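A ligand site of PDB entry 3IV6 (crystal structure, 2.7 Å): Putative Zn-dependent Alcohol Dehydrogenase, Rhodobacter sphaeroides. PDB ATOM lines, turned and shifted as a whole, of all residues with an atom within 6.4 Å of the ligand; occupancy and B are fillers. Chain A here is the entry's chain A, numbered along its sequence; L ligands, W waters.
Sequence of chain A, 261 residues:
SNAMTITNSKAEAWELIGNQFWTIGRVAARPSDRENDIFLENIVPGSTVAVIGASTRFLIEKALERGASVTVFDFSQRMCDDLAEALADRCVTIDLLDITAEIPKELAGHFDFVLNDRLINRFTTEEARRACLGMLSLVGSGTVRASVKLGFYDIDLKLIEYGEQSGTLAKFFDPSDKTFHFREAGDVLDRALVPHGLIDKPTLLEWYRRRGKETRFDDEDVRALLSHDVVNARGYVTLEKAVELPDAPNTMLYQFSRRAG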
ATOM      1  N   ASN A   8      -8.475  -1.420   5.285  1.00  0.00           N
ATOM      2  CA  ASN A   8      -8.920  -2.145   6.468  1.00  0.00           C
ATOM      3  C   ASN A   8      -8.325  -3.536   6.625  1.00  0.00           C
ATOM      4  O   ASN A   8      -8.883  -4.516   6.190  1.00  0.00           O
ATOM      5  CB  ASN A   8     -10.439  -2.244   6.482  1.00  0.00           C
ATOM      6  CG  ASN A   8     -10.992  -2.482   7.865  1.00  0.00           C
ATOM      7  OD1 ASN A   8     -10.280  -2.919   8.765  1.00  0.00           O
ATOM      8  ND2 ASN A   8     -12.266  -2.177   8.051  1.00  0.00           N
ATOM      9  N   LYS A  10      -8.265  -5.415   9.027  1.00  0.00           N
ATOM     10  CA  LYS A  10      -9.034  -6.345   9.863  1.00  0.00           C
ATOM     11  C   LYS A  10      -9.641  -7.449   9.001  1.00  0.00           C
ATOM     12  O   LYS A  10      -9.783  -8.576   9.461  1.00  0.00           O
ATOM     13  CB  LYS A  10     -10.113  -5.642  10.668  1.00  0.00           C
ATOM     14  CG  LYS A  10      -9.554  -4.801  11.760  1.00  0.00           C
ATOM     15  CD  LYS A  10     -10.647  -4.179  12.614  1.00  0.00           C
ATOM     16  CE  LYS A  10     -10.072  -3.644  13.901  1.00  0.00           C
ATOM     17  NZ  LYS A  10     -11.071  -3.210  14.902  1.00  0.00           N
ATOM     18  N   ALA A  11      -9.969  -7.132   7.744  1.00  0.00           N
ATOM     19  CA  ALA A  11     -10.525  -8.164   6.884  1.00  0.00           C
ATOM     20  C   ALA A  11      -9.585  -9.387   6.804  1.00  0.00           C
ATOM     21  O   ALA A  11     -10.052 -10.525   6.707  1.00  0.00           O
ATOM     22  CB  ALA A  11     -10.870  -7.618   5.502  1.00  0.00           C
ATOM     23  N   TRP A  14     -10.377 -12.325   8.942  1.00  0.00           N
ATOM     24  CA  TRP A  14     -11.484 -13.237   8.677  1.00  0.00           C
ATOM     25  C   TRP A  14     -11.270 -14.177   7.463  1.00  0.00           C
ATOM     26  O   TRP A  14     -11.969 -15.170   7.296  1.00  0.00           O
ATOM     27  CB  TRP A  14     -12.816 -12.480   8.651  1.00  0.00           C
ATOM     28  CG  TRP A  14     -13.049 -11.725   9.918  1.00  0.00           C
ATOM     29  CD1 TRP A  14     -12.583 -10.481  10.232  1.00  0.00           C
ATOM     30  CD2 TRP A  14     -13.804 -12.160  11.062  1.00  0.00           C
ATOM     31  NE1 TRP A  14     -13.005 -10.114  11.492  1.00  0.00           N
ATOM     32  CE2 TRP A  14     -13.757 -11.117  12.021  1.00  0.00           C
ATOM     33  CE3 TRP A  14     -14.550 -13.315  11.355  1.00  0.00           C
ATOM     34  CZ2 TRP A  14     -14.420 -11.205  13.257  1.00  0.00           C
ATOM     35  CZ3 TRP A  14     -15.194 -13.405  12.581  1.00  0.00           C
ATOM     36  CH2 TRP A  14     -15.119 -12.354  13.522  1.00  0.00           C
ATOM     37  N   PHE A  21     -16.237 -20.363  11.622  1.00  0.00           N
ATOM     38  CA  PHE A  21     -16.943 -19.620  12.640  1.00  0.00           C
ATOM     39  C   PHE A  21     -18.297 -20.211  13.040  1.00  0.00           C
ATOM     40  O   PHE A  21     -18.651 -20.233  14.218  1.00  0.00           O
ATOM     41  CB  PHE A  21     -17.116 -18.164  12.246  1.00  0.00           C
ATOM     42  CG  PHE A  21     -17.636 -17.348  13.379  1.00  0.00           C
ATOM     43  CD1 PHE A  21     -16.757 -16.811  14.307  1.00  0.00           C
ATOM     44  CD2 PHE A  21     -19.011 -17.182  13.569  1.00  0.00           C
ATOM     45  CE1 PHE A  21     -17.211 -16.076  15.381  1.00  0.00           C
ATOM     46  CE2 PHE A  21     -19.491 -16.463  14.666  1.00  0.00           C
ATOM     47  CZ  PHE A  21     -18.588 -15.901  15.566  1.00  0.00           C
ATOM     48  N   ALA A  29     -21.405 -17.700  20.348  1.00  0.00           N
ATOM     49  CA  ALA A  29     -20.851 -16.510  19.747  1.00  0.00           C
ATOM     50  C   ALA A  29     -21.731 -16.118  18.552  1.00  0.00           C
ATOM     51  O   ALA A  29     -21.482 -15.110  17.893  1.00  0.00           O
ATOM     52  CB  ALA A  29     -19.391 -16.733  19.332  1.00  0.00           C
ATOM     53  N   ARG A  30     -22.734 -16.925  18.268  1.00  0.00           N
ATOM     54  CA  ARG A  30     -23.728 -16.583  17.269  1.00  0.00           C
ATOM     55  C   ARG A  30     -25.105 -16.553  17.904  1.00  0.00           C
ATOM     56  O   ARG A  30     -25.293 -17.092  18.991  1.00  0.00           O
ATOM     57  CB  ARG A  30     -23.722 -17.572  16.125  1.00  0.00           C
ATOM     58  CG  ARG A  30     -24.019 -18.955  16.509  1.00  0.00           C
ATOM     59  CD  ARG A  30     -24.492 -19.710  15.294  1.00  0.00           C
ATOM     60  NE  ARG A  30     -24.566 -21.163  15.482  1.00  0.00           N
ATOM     61  CZ  ARG A  30     -23.506 -21.956  15.583  1.00  0.00           C
ATOM     62  NH1 ARG A  30     -22.276 -21.428  15.539  1.00  0.00           N
ATOM     63  NH2 ARG A  30     -23.673 -23.276  15.751  1.00  0.00           N
ATOM     64  N   PRO A  31     -26.083 -15.922  17.244  1.00  0.00           N
ATOM     65  CA  PRO A  31     -27.407 -15.975  17.880  1.00  0.00           C
ATOM     66  C   PRO A  31     -27.946 -17.384  17.971  1.00  0.00           C
ATOM     67  O   PRO A  31     -27.713 -18.189  17.095  1.00  0.00           O
ATOM     68  CB  PRO A  31     -28.276 -15.096  16.963  1.00  0.00           C
ATOM     69  CG  PRO A  31     -27.294 -14.281  16.157  1.00  0.00           C
ATOM     70  CD  PRO A  31     -26.063 -15.091  16.031  1.00  0.00           C
ATOM     71  N   ILE A  52     -25.316  -7.266   7.859  1.00  0.00           N
ATOM     72  CA  ILE A  52     -23.885  -7.048   7.938  1.00  0.00           C
ATOM     73  C   ILE A  52     -23.192  -8.154   8.715  1.00  0.00           C
ATOM     74  O   ILE A  52     -23.496  -8.383   9.888  1.00  0.00           O
ATOM     75  CB  ILE A  52     -23.553  -5.684   8.580  1.00  0.00           C
ATOM     76  CG1 ILE A  52     -24.533  -4.620   8.092  1.00  0.00           C
ATOM     77  CG2 ILE A  52     -22.121  -5.284   8.269  1.00  0.00           C
ATOM     78  CD1 ILE A  52     -24.597  -4.488   6.590  1.00  0.00           C
ATOM     79  N   GLY A  53     -22.260  -8.842   8.068  1.00  0.00           N
ATOM     80  CA  GLY A  53     -21.590  -9.986   8.670  1.00  0.00           C
ATOM     81  C   GLY A  53     -22.011 -11.295   8.032  1.00  0.00           C
ATOM     82  O   GLY A  53     -22.983 -11.913   8.451  1.00  0.00           O
ATOM     83  N   ALA A  54     -21.260 -11.718   7.019  1.00  0.00           N
ATOM     84  CA  ALA A  54     -21.579 -12.944   6.306  1.00  0.00           C
ATOM     85  C   ALA A  54     -21.364 -14.170   7.191  1.00  0.00           C
ATOM     86  O   ALA A  54     -21.633 -15.300   6.780  1.00  0.00           O
ATOM     87  CB  ALA A  54     -20.737 -13.058   5.046  1.00  0.00           C
ATOM     88  N   SER A  55     -20.877 -13.936   8.403  1.00  0.00           N
ATOM     89  CA  SER A  55     -20.596 -15.021   9.342  1.00  0.00           C
ATOM     90  C   SER A  55     -21.871 -15.531  10.007  1.00  0.00           C
ATOM     91  O   SER A  55     -21.941 -16.666  10.470  1.00  0.00           O
ATOM     92  CB  SER A  55     -19.598 -14.569  10.400  1.00  0.00           C
ATOM     93  OG  SER A  55     -20.198 -13.655  11.312  1.00  0.00           O
ATOM     94  N   THR A  56     -22.896 -14.679  10.032  1.00  0.00           N
ATOM     95  CA  THR A  56     -24.167 -15.017  10.687  1.00  0.00           C
ATOM     96  C   THR A  56     -25.084 -15.850   9.775  1.00  0.00           C
ATOM     97  O   THR A  56     -26.218 -15.448   9.420  1.00  0.00           O
ATOM     98  CB  THR A  56     -24.919 -13.776  11.208  1.00  0.00           C
ATOM     99  OG1 THR A  56     -23.978 -12.738  11.505  1.00  0.00           O
ATOM    100  CG2 THR A  56     -25.676 -14.098  12.482  1.00  0.00           C
ATOM    101  N   ARG A  57     -24.580 -17.042   9.464  1.00  0.00           N
ATOM    102  CA  ARG A  57     -25.184 -17.913   8.474  1.00  0.00           C
ATOM    103  C   ARG A  57     -26.605 -18.394   8.786  1.00  0.00           C
ATOM    104  O   ARG A  57     -27.393 -18.582   7.856  1.00  0.00           O
ATOM    105  CB  ARG A  57     -24.253 -19.093   8.192  1.00  0.00           C
ATOM    106  CG  ARG A  57     -24.832 -20.070   7.195  1.00  0.00           C
ATOM    107  CD  ARG A  57     -25.353 -21.275   7.898  1.00  0.00           C
ATOM    108  NE  ARG A  57     -26.128 -22.104   6.980  1.00  0.00           N
ATOM    109  CZ  ARG A  57     -25.712 -23.264   6.477  1.00  0.00           C
ATOM    110  NH1 ARG A  57     -24.534 -23.778   6.805  1.00  0.00           N
ATOM    111  NH2 ARG A  57     -26.505 -23.909   5.636  1.00  0.00           N
ATOM    112  N   PHE A  73     -23.695  -8.124   3.491  1.00  0.00           N
ATOM    113  CA  PHE A  73     -22.487  -7.325   3.331  1.00  0.00           C
ATOM    114  C   PHE A  73     -21.394  -7.849   4.250  1.00  0.00           C
ATOM    115  O   PHE A  73     -21.646  -8.175   5.398  1.00  0.00           O
ATOM    116  CB  PHE A  73     -22.754  -5.871   3.641  1.00  0.00           C
ATOM    117  CG  PHE A  73     -23.724  -5.231   2.696  1.00  0.00           C
ATOM    118  CD1 PHE A  73     -23.431  -5.145   1.330  1.00  0.00           C
ATOM    119  CD2 PHE A  73     -24.950  -4.702   3.143  1.00  0.00           C
ATOM    120  CE1 PHE A  73     -24.295  -4.548   0.454  1.00  0.00           C
ATOM    121  CE2 PHE A  73     -25.858  -4.104   2.245  1.00  0.00           C
ATOM    122  CZ  PHE A  73     -25.519  -4.027   0.906  1.00  0.00           C
ATOM    123  N   ASP A  74     -20.190  -7.928   3.732  1.00  0.00           N
ATOM    124  CA  ASP A  74     -19.043  -8.356   4.533  1.00  0.00           C
ATOM    125  C   ASP A  74     -17.755  -7.832   3.906  1.00  0.00           C
ATOM    126  O   ASP A  74     -17.647  -7.705   2.672  1.00  0.00           O
ATOM    127  CB  ASP A  74     -18.995  -9.893   4.617  1.00  0.00           C
ATOM    128  CG  ASP A  74     -18.201 -10.384   5.815  1.00  0.00           C
ATOM    129  OD1 ASP A  74     -16.963 -10.227   5.819  1.00  0.00           O
ATOM    130  OD2 ASP A  74     -18.845 -10.896   6.770  1.00  0.00           O
ATOM    131  N   PHE A  75     -16.773  -7.511   4.752  1.00  0.00           N
ATOM    132  CA  PHE A  75     -15.530  -6.945   4.229  1.00  0.00           C
ATOM    133  C   PHE A  75     -14.440  -7.980   3.915  1.00  0.00           C
ATOM    134  O   PHE A  75     -13.302  -7.617   3.646  1.00  0.00           O
ATOM    135  CB  PHE A  75     -15.029  -5.798   5.103  1.00  0.00           C
ATOM    136  CG  PHE A  75     -14.408  -6.232   6.376  1.00  0.00           C
ATOM    137  CD1 PHE A  75     -14.565  -7.544   6.831  1.00  0.00           C
ATOM    138  CD2 PHE A  75     -13.680  -5.344   7.132  1.00  0.00           C
ATOM    139  CE1 PHE A  75     -13.995  -7.969   8.019  1.00  0.00           C
ATOM    140  CE2 PHE A  75     -13.110  -5.764   8.328  1.00  0.00           C
ATOM    141  CZ  PHE A  75     -13.277  -7.088   8.767  1.00  0.00           C
ATOM    142  N   SER A  76     -14.802  -9.243   3.949  1.00  0.00           N
ATOM    143  CA  SER A  76     -13.882 -10.360   3.735  1.00  0.00           C
ATOM    144  C   SER A  76     -14.287 -11.273   2.567  1.00  0.00           C
ATOM    145  O   SER A  76     -15.423 -11.711   2.472  1.00  0.00           O
ATOM    146  CB  SER A  76     -13.732 -11.183   5.020  1.00  0.00           C
ATOM    147  OG  SER A  76     -13.508 -12.548   4.716  1.00  0.00           O
ATOM    148  N   MET A  79     -15.228 -15.061   3.632  1.00  0.00           N
ATOM    149  CA  MET A  79     -16.513 -15.064   4.318  1.00  0.00           C
ATOM    150  C   MET A  79     -17.649 -15.064   3.331  1.00  0.00           C
ATOM    151  O   MET A  79     -18.481 -15.963   3.367  1.00  0.00           O
ATOM    152  CB  MET A  79     -16.600 -13.911   5.308  1.00  0.00           C
ATOM    153  CG  MET A  79     -15.934 -14.277   6.621  1.00  0.00           C
ATOM    154  SD  MET A  79     -16.809 -15.836   7.511  1.00  0.00           S
ATOM    155  CE  MET A  79     -15.737 -15.733   9.150  1.00  0.00           C
ATOM    156  N   LEU A  97     -18.354  -5.481   1.116  1.00  0.00           N
ATOM    157  CA  LEU A  97     -18.498  -4.086   1.541  1.00  0.00           C
ATOM    158  C   LEU A  97     -17.968  -3.848   2.962  1.00  0.00           C
ATOM    159  O   LEU A  97     -18.041  -4.730   3.809  1.00  0.00           O
ATOM    160  CB  LEU A  97     -19.962  -3.619   1.413  1.00  0.00           C
ATOM    161  CG  LEU A  97     -20.378  -2.208   1.881  1.00  0.00           C
ATOM    162  CD1 LEU A  97     -21.571  -1.702   1.127  1.00  0.00           C
ATOM    163  CD2 LEU A  97     -20.677  -2.135   3.397  1.00  0.00           C
ATOM    164  N   ASP A  98     -17.442  -2.654   3.210  1.00  0.00           N
ATOM    165  CA  ASP A  98     -16.930  -2.363   4.529  1.00  0.00           C
ATOM    166  C   ASP A  98     -17.813  -1.333   5.238  1.00  0.00           C
ATOM    167  O   ASP A  98     -17.731  -0.142   4.963  1.00  0.00           O
ATOM    168  CB  ASP A  98     -15.508  -1.872   4.432  1.00  0.00           C
ATOM    169  CG  ASP A  98     -14.948  -1.400   5.780  1.00  0.00           C
ATOM    170  OD1 ASP A  98     -15.719  -1.232   6.749  1.00  0.00           O
ATOM    171  OD2 ASP A  98     -13.711  -1.174   5.860  1.00  0.00           O
ATOM    172  N   ILE A  99     -18.640  -1.789   6.174  1.00  0.00           N
ATOM    173  CA  ILE A  99     -19.572  -0.893   6.814  1.00  0.00           C
ATOM    174  C   ILE A  99     -18.986   0.353   7.485  1.00  0.00           C
ATOM    175  O   ILE A  99     -19.726   1.272   7.779  1.00  0.00           O
ATOM    176  CB  ILE A  99     -20.482  -1.633   7.818  1.00  0.00           C
ATOM    177  CG1 ILE A  99     -21.771  -0.819   8.072  1.00  0.00           C
ATOM    178  CG2 ILE A  99     -19.746  -1.956   9.080  1.00  0.00           C
ATOM    179  CD1 ILE A  99     -22.857  -1.054   7.049  1.00  0.00           C
ATOM    180  N   THR A 100     -17.678   0.409   7.712  1.00  0.00           N
ATOM    181  CA  THR A 100     -17.064   1.641   8.251  1.00  0.00           C
ATOM    182  C   THR A 100     -16.583   2.599   7.149  1.00  0.00           C
ATOM    183  O   THR A 100     -16.091   3.695   7.423  1.00  0.00           O
ATOM    184  CB  THR A 100     -15.864   1.341   9.150  1.00  0.00           C
ATOM    185  OG1 THR A 100     -14.792   0.880   8.315  1.00  0.00           O
ATOM    186  CG2 THR A 100     -16.205   0.287  10.201  1.00  0.00           C
ATOM    187  N   ALA A 101     -16.705   2.142   5.910  1.00  0.00           N
ATOM    188  CA  ALA A 101     -16.423   2.958   4.758  1.00  0.00           C
ATOM    189  C   ALA A 101     -17.719   3.647   4.328  1.00  0.00           C
ATOM    190  O   ALA A 101     -18.825   3.229   4.712  1.00  0.00           O
ATOM    191  CB  ALA A 101     -15.896   2.098   3.628  1.00  0.00           C
ATOM    192  N   ASN A 116     -27.403  -6.723  12.462  1.00  0.00           N
ATOM    193  CA  ASN A 116     -26.127  -7.374  12.765  1.00  0.00           C
ATOM    194  C   ASN A 116     -26.003  -7.822  14.211  1.00  0.00           C
ATOM    195  O   ASN A 116     -26.537  -7.156  15.119  1.00  0.00           O
ATOM    196  CB  ASN A 116     -24.938  -6.501  12.339  1.00  0.00           C
ATOM    197  CG  ASN A 116     -25.023  -5.071  12.882  1.00  0.00           C
ATOM    198  OD1 ASN A 116     -25.504  -4.176  12.191  1.00  0.00           O
ATOM    199  ND2 ASN A 116     -24.505  -4.851  14.079  1.00  0.00           N
ATOM    200  N   ASP A 117     -25.321  -8.942  14.413  1.00  0.00           N
ATOM    201  CA  ASP A 117     -25.142  -9.508  15.742  1.00  0.00           C
ATOM    202  C   ASP A 117     -23.714  -9.359  16.260  1.00  0.00           C
ATOM    203  O   ASP A 117     -22.832 -10.089  15.837  1.00  0.00           O
ATOM    204  CB  ASP A 117     -25.515 -10.991  15.768  1.00  0.00           C
ATOM    205  CG  ASP A 117     -25.382 -11.604  17.173  1.00  0.00           C
ATOM    206  OD1 ASP A 117     -25.691 -10.933  18.189  1.00  0.00           O
ATOM    207  OD2 ASP A 117     -24.979 -12.779  17.263  1.00  0.00           O
ATOM    208  N   ARG A 118     -23.519  -8.440  17.196  1.00  0.00           N
ATOM    209  CA  ARG A 118     -22.245  -8.275  17.895  1.00  0.00           C
ATOM    210  C   ARG A 118     -21.088  -7.851  16.969  1.00  0.00           C
ATOM    211  O   ARG A 118     -19.902  -8.130  17.213  1.00  0.00           O
ATOM    212  CB  ARG A 118     -21.915  -9.536  18.680  1.00  0.00           C
ATOM    213  CG  ARG A 118     -22.691  -9.627  19.992  1.00  0.00           C
ATOM    214  CD  ARG A 118     -22.531 -10.973  20.693  1.00  0.00           C
ATOM    215  NE  ARG A 118     -23.349 -12.060  20.153  1.00  0.00           N
ATOM    216  CZ  ARG A 118     -23.271 -13.329  20.576  1.00  0.00           C
ATOM    217  NH1 ARG A 118     -22.402 -13.626  21.516  1.00  0.00           N
ATOM    218  NH2 ARG A 118     -24.031 -14.310  20.053  1.00  0.00           N
ATOM    219  N   LEU A 119     -21.452  -7.116  15.929  1.00  0.00           N
ATOM    220  CA  LEU A 119     -20.495  -6.612  14.948  1.00  0.00           C
ATOM    221  C   LEU A 119     -19.799  -5.380  15.497  1.00  0.00           C
ATOM    222  O   LEU A 119     -18.666  -5.094  15.181  1.00  0.00           O
ATOM    223  CB  LEU A 119     -21.269  -6.231  13.698  1.00  0.00           C
ATOM    224  CG  LEU A 119     -20.517  -5.378  12.700  1.00  0.00           C
ATOM    225  CD1 LEU A 119     -19.312  -6.170  12.178  1.00  0.00           C
ATOM    226  CD2 LEU A 119     -21.446  -4.934  11.591  1.00  0.00           C
ATOM    227  N   ILE A 120     -20.490  -4.651  16.348  1.00  0.00           N
ATOM    228  CA  ILE A 120     -19.984  -3.424  16.916  1.00  0.00           C
ATOM    229  C   ILE A 120     -18.837  -3.743  17.862  1.00  0.00           C
ATOM    230  O   ILE A 120     -17.993  -2.906  18.132  1.00  0.00           O
ATOM    231  CB  ILE A 120     -21.141  -2.628  17.609  1.00  0.00           C
ATOM    232  CG1 ILE A 120     -21.976  -1.850  16.589  1.00  0.00           C
ATOM    233  CG2 ILE A 120     -20.614  -1.606  18.639  1.00  0.00           C
ATOM    234  CD1 ILE A 120     -23.376  -1.659  17.045  1.00  0.00           C
ATOM    235  N   ARG A 122     -16.543  -5.648  17.191  1.00  0.00           N
ATOM    236  CA  ARG A 122     -15.392  -5.763  16.333  1.00  0.00           C
ATOM    237  C   ARG A 122     -14.837  -4.409  15.948  1.00  0.00           C
ATOM    238  O   ARG A 122     -13.938  -4.327  15.094  1.00  0.00           O
ATOM    239  CB  ARG A 122     -15.712  -6.561  15.070  1.00  0.00           C
ATOM    240  CG  ARG A 122     -16.020  -8.047  15.306  1.00  0.00           C
ATOM    241  CD  ARG A 122     -15.191  -8.598  16.470  1.00  0.00           C
ATOM    242  NE  ARG A 122     -16.049  -9.346  17.384  1.00  0.00           N
ATOM    243  CZ  ARG A 122     -16.036  -9.266  18.702  1.00  0.00           C
ATOM    244  NH1 ARG A 122     -15.174  -8.490  19.323  1.00  0.00           N
ATOM    245  NH2 ARG A 122     -16.890  -9.987  19.402  1.00  0.00           N
ATOM    246  N   PHE A 123     -15.343  -3.357  16.600  1.00  0.00           N
ATOM    247  CA  PHE A 123     -14.878  -1.994  16.340  1.00  0.00           C
ATOM    248  C   PHE A 123     -14.208  -1.295  17.514  1.00  0.00           C
ATOM    249  O   PHE A 123     -14.393  -1.636  18.693  1.00  0.00           O
ATOM    250  CB  PHE A 123     -16.029  -1.088  15.846  1.00  0.00           C
ATOM    251  CG  PHE A 123     -16.758  -1.622  14.632  1.00  0.00           C
ATOM    252  CD1 PHE A 123     -16.066  -2.225  13.577  1.00  0.00           C
ATOM    253  CD2 PHE A 123     -18.142  -1.472  14.540  1.00  0.00           C
ATOM    254  CE1 PHE A 123     -16.717  -2.721  12.479  1.00  0.00           C
ATOM    255  CE2 PHE A 123     -18.817  -1.956  13.412  1.00  0.00           C
ATOM    256  CZ  PHE A 123     -18.078  -2.600  12.370  1.00  0.00           C
ATOM    257  N   GLU A 127     -14.453   3.743  14.896  1.00  0.00           N
ATOM    258  CA  GLU A 127     -14.900   2.815  13.877  1.00  0.00           C
ATOM    259  C   GLU A 127     -16.425   2.523  14.044  1.00  0.00           C
ATOM    260  O   GLU A 127     -17.199   2.565  13.080  1.00  0.00           O
ATOM    261  CB  GLU A 127     -14.114   1.517  13.963  1.00  0.00           C
ATOM    262  CG  GLU A 127     -12.910   1.392  13.110  1.00  0.00           C
ATOM    263  CD  GLU A 127     -12.470  -0.084  12.960  1.00  0.00           C
ATOM    264  OE1 GLU A 127     -12.275  -0.777  13.991  1.00  0.00           O
ATOM    265  OE2 GLU A 127     -12.316  -0.567  11.799  1.00  0.00           O
HETATM  266  N1  LIG L   1     -19.566 -13.173  13.878  1.00  0.00           N
HETATM  267  C1  LIG L   1     -20.437 -13.018  15.020  1.00  0.00           C
HETATM  268  C2  LIG L   1     -21.835 -13.497  14.712  1.00  0.00           C
HETATM  269  O1  LIG L   1     -22.180 -13.934  13.606  1.00  0.00           O
HETATM  270  O2  LIG L   1     -22.625 -13.445  15.634  1.00  0.00           O
HETATM  271  C3  LIG L   1     -20.408 -11.598  15.566  1.00  0.00           C
HETATM  272  C4  LIG L   1     -19.300 -10.698  14.997  1.00  0.00           C
HETATM  273  S1  LIG L   1     -19.602  -9.936  13.366  1.00  0.00           S
HETATM  274  C5  LIG L   1     -21.168 -10.691  12.832  1.00  0.00           C
HETATM  275  C6  LIG L   1     -18.285 -10.643  12.312  1.00  0.00           C
HETATM  276  C7  LIG L   1     -18.512 -10.721  10.813  1.00  0.00           C
HETATM  277  O3  LIG L   1     -18.629  -9.412  10.272  1.00  0.00           O
HETATM  278  C8  LIG L   1     -17.364 -11.365  10.063  1.00  0.00           C
HETATM  279  O4  LIG L   1     -17.922 -12.112   9.008  1.00  0.00           O
HETATM  280  C9  LIG L   1     -16.602 -10.202   9.461  1.00  0.00           C
HETATM  281  O5  LIG L   1     -16.043 -10.540   8.203  1.00  0.00           O
HETATM  282  C10 LIG L   1     -17.671  -9.140   9.280  1.00  0.00           C
HETATM  283  N2  LIG L   1     -17.121  -7.786   9.490  1.00  0.00           N
HETATM  284  C11 LIG L   1     -16.331  -7.390  10.529  1.00  0.00           C
HETATM  285  N3  LIG L   1     -16.011  -6.079  10.351  1.00  0.00           N
HETATM  286  C12 LIG L   1     -16.601  -5.617   9.212  1.00  0.00           C
HETATM  287  C13 LIG L   1     -16.608  -4.366   8.575  1.00  0.00           C
HETATM  288  N4  LIG L   1     -15.945  -3.311   9.057  1.00  0.00           N
HETATM  289  N5  LIG L   1     -17.297  -4.235   7.392  1.00  0.00           N
HETATM  290  C14 LIG L   1     -17.949  -5.341   6.860  1.00  0.00           C
HETATM  291  N6  LIG L   1     -17.968  -6.561   7.478  1.00  0.00           N
HETATM  292  C15 LIG L   1     -17.299  -6.706   8.646  1.00  0.00           C
HETATM  293  O   HOH W   1     -13.512  -2.794  10.671  1.00  0.00           O
HETATM  294  O   HOH W   2     -13.934  -5.316  12.106  1.00  0.00           O
HETATM  295  O   HOH W   3     -22.926 -16.453  13.494  1.00  0.00           O
HETATM  296  O   HOH W   4     -24.261 -10.021  11.756  1.00  0.00           O
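Water W3 bridges an oxygen (O1) of the ligand and the backbone carbonyl oxygen of Ser 55. Water W2 lies within hydrogen-bond range of N3 of the ligand (2.8 Å) and O of Arg 122 (3.1 Å). Water W1 lies within hydrogen-bond range of the side-chain carboxylate (OE2) of Glu 127, a nitrogen (N4) of the ligand and the side-chain amide nitrogen (ND2) of Asn 8. Water W4 lies within hydrogen-bond range of the backbone carbonyl oxygen (O) of Ile 52, the side-chain hydroxyl (OG1) of Thr 56 and the backbone NH (N) of Asp 117.
Asn 8 touches the ligand. Trp 14 touches the ligand (CG to O5, 3.6 Å). CZ of Phe 21 touches N1 of the ligand, 3.4 Å away. CA of Arg 30 touches O2 of the ligand, 3.7 Å away. Pro 31 touches the ligand. Gly 53 touches the ligand. N of Ala 54 touches O4 of the ligand, 3.9 Å away. CB of Ser 76 touches O5 of the ligand, at 3.99 Å. Met 79 touches the ligand. O of Leu 97 touches C14 of the ligand, at 3.1 Å. CG2 of Thr 100 touches N4 of the ligand, 3.8 Å away. O of Arg 118 touches C4 of the ligand, at 3.4 Å. Leu 119 touches the ligand. Phe 123 touches the ligand. Hydrophobic or aromatic side chains within 4 Å of the ligand: Trp 14, Phe 21, Pro 31, Phe 75, Met 79, Ile 99, Leu 119 and Phe 123. Within 4 Å of the ligand: Asn 8, Trp 14, Phe 21, Ala 29, Arg 30, Pro 31, Gly 53, Ala 54, Ser 55, Thr 56, Asp 74, Phe 75, Ser 76, Met 79, Leu 97, Asp 98, Ile 99, Thr 100, Asp 117, Arg 118, Leu 119 and Phe 123. The nearest printed residue that does not touch the ligand is Arg 122 (4.2 Å).
O5 of the ligand lies within hydrogen-bond range of OD1 of Asp 74 (2.6 Å). The side-chain hydroxyl of Ser 55 is in hydrogen-bond range of a nitrogen (N1) of the ligand. OD2 of Asp 117 sits close to O2 of the ligand (2.9 Å). The side-chain hydroxyl of Thr 56 is in hydrogen-bond range of an oxygen (O1) of the ligand, at 3.0 Å. O of Ala 29 sits close to O2 of the ligand (3.0 Å). N of Ile 99 sits at hydrogen-bond distance from N5 of the ligand (3.0 Å). A nitrogen (N4) of the ligand sits at hydrogen-bond distance from the side-chain carboxylate of Asp 98 (3.1 Å). The backbone NH of Phe 75 sits at hydrogen-bond distance from a nitrogen (N6) of the ligand (3.1 Å).
N of Ala 54 lies within hydrogen-bond range of OD2 of Asp 74 (2.6 Å). The backbone NH of Ser 76 sits at hydrogen-bond distance from the side-chain carboxylate of Asp 74 (3.0 Å). NH2 of Arg 118 sits close to O of Ala 29 (3.4 Å). The backbone carbonyl oxygen (O) of Leu 97 sits at hydrogen-bond distance from the backbone NH (N) of Phe 75 (3.2 Å). OD1 of Asp 98 is in hydrogen-bond range of N of Thr 100. N of Gly 53 is in hydrogen-bond range of O of Phe 73. The backbone carbonyl oxygen of Arg 30 lies within hydrogen-bond range of the guanidinium group of Arg 118 (3.2 Å). The side-chain amide oxygen of Asn 8 sits close to the backbone NH of Lys 10, 3.2 Å away.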
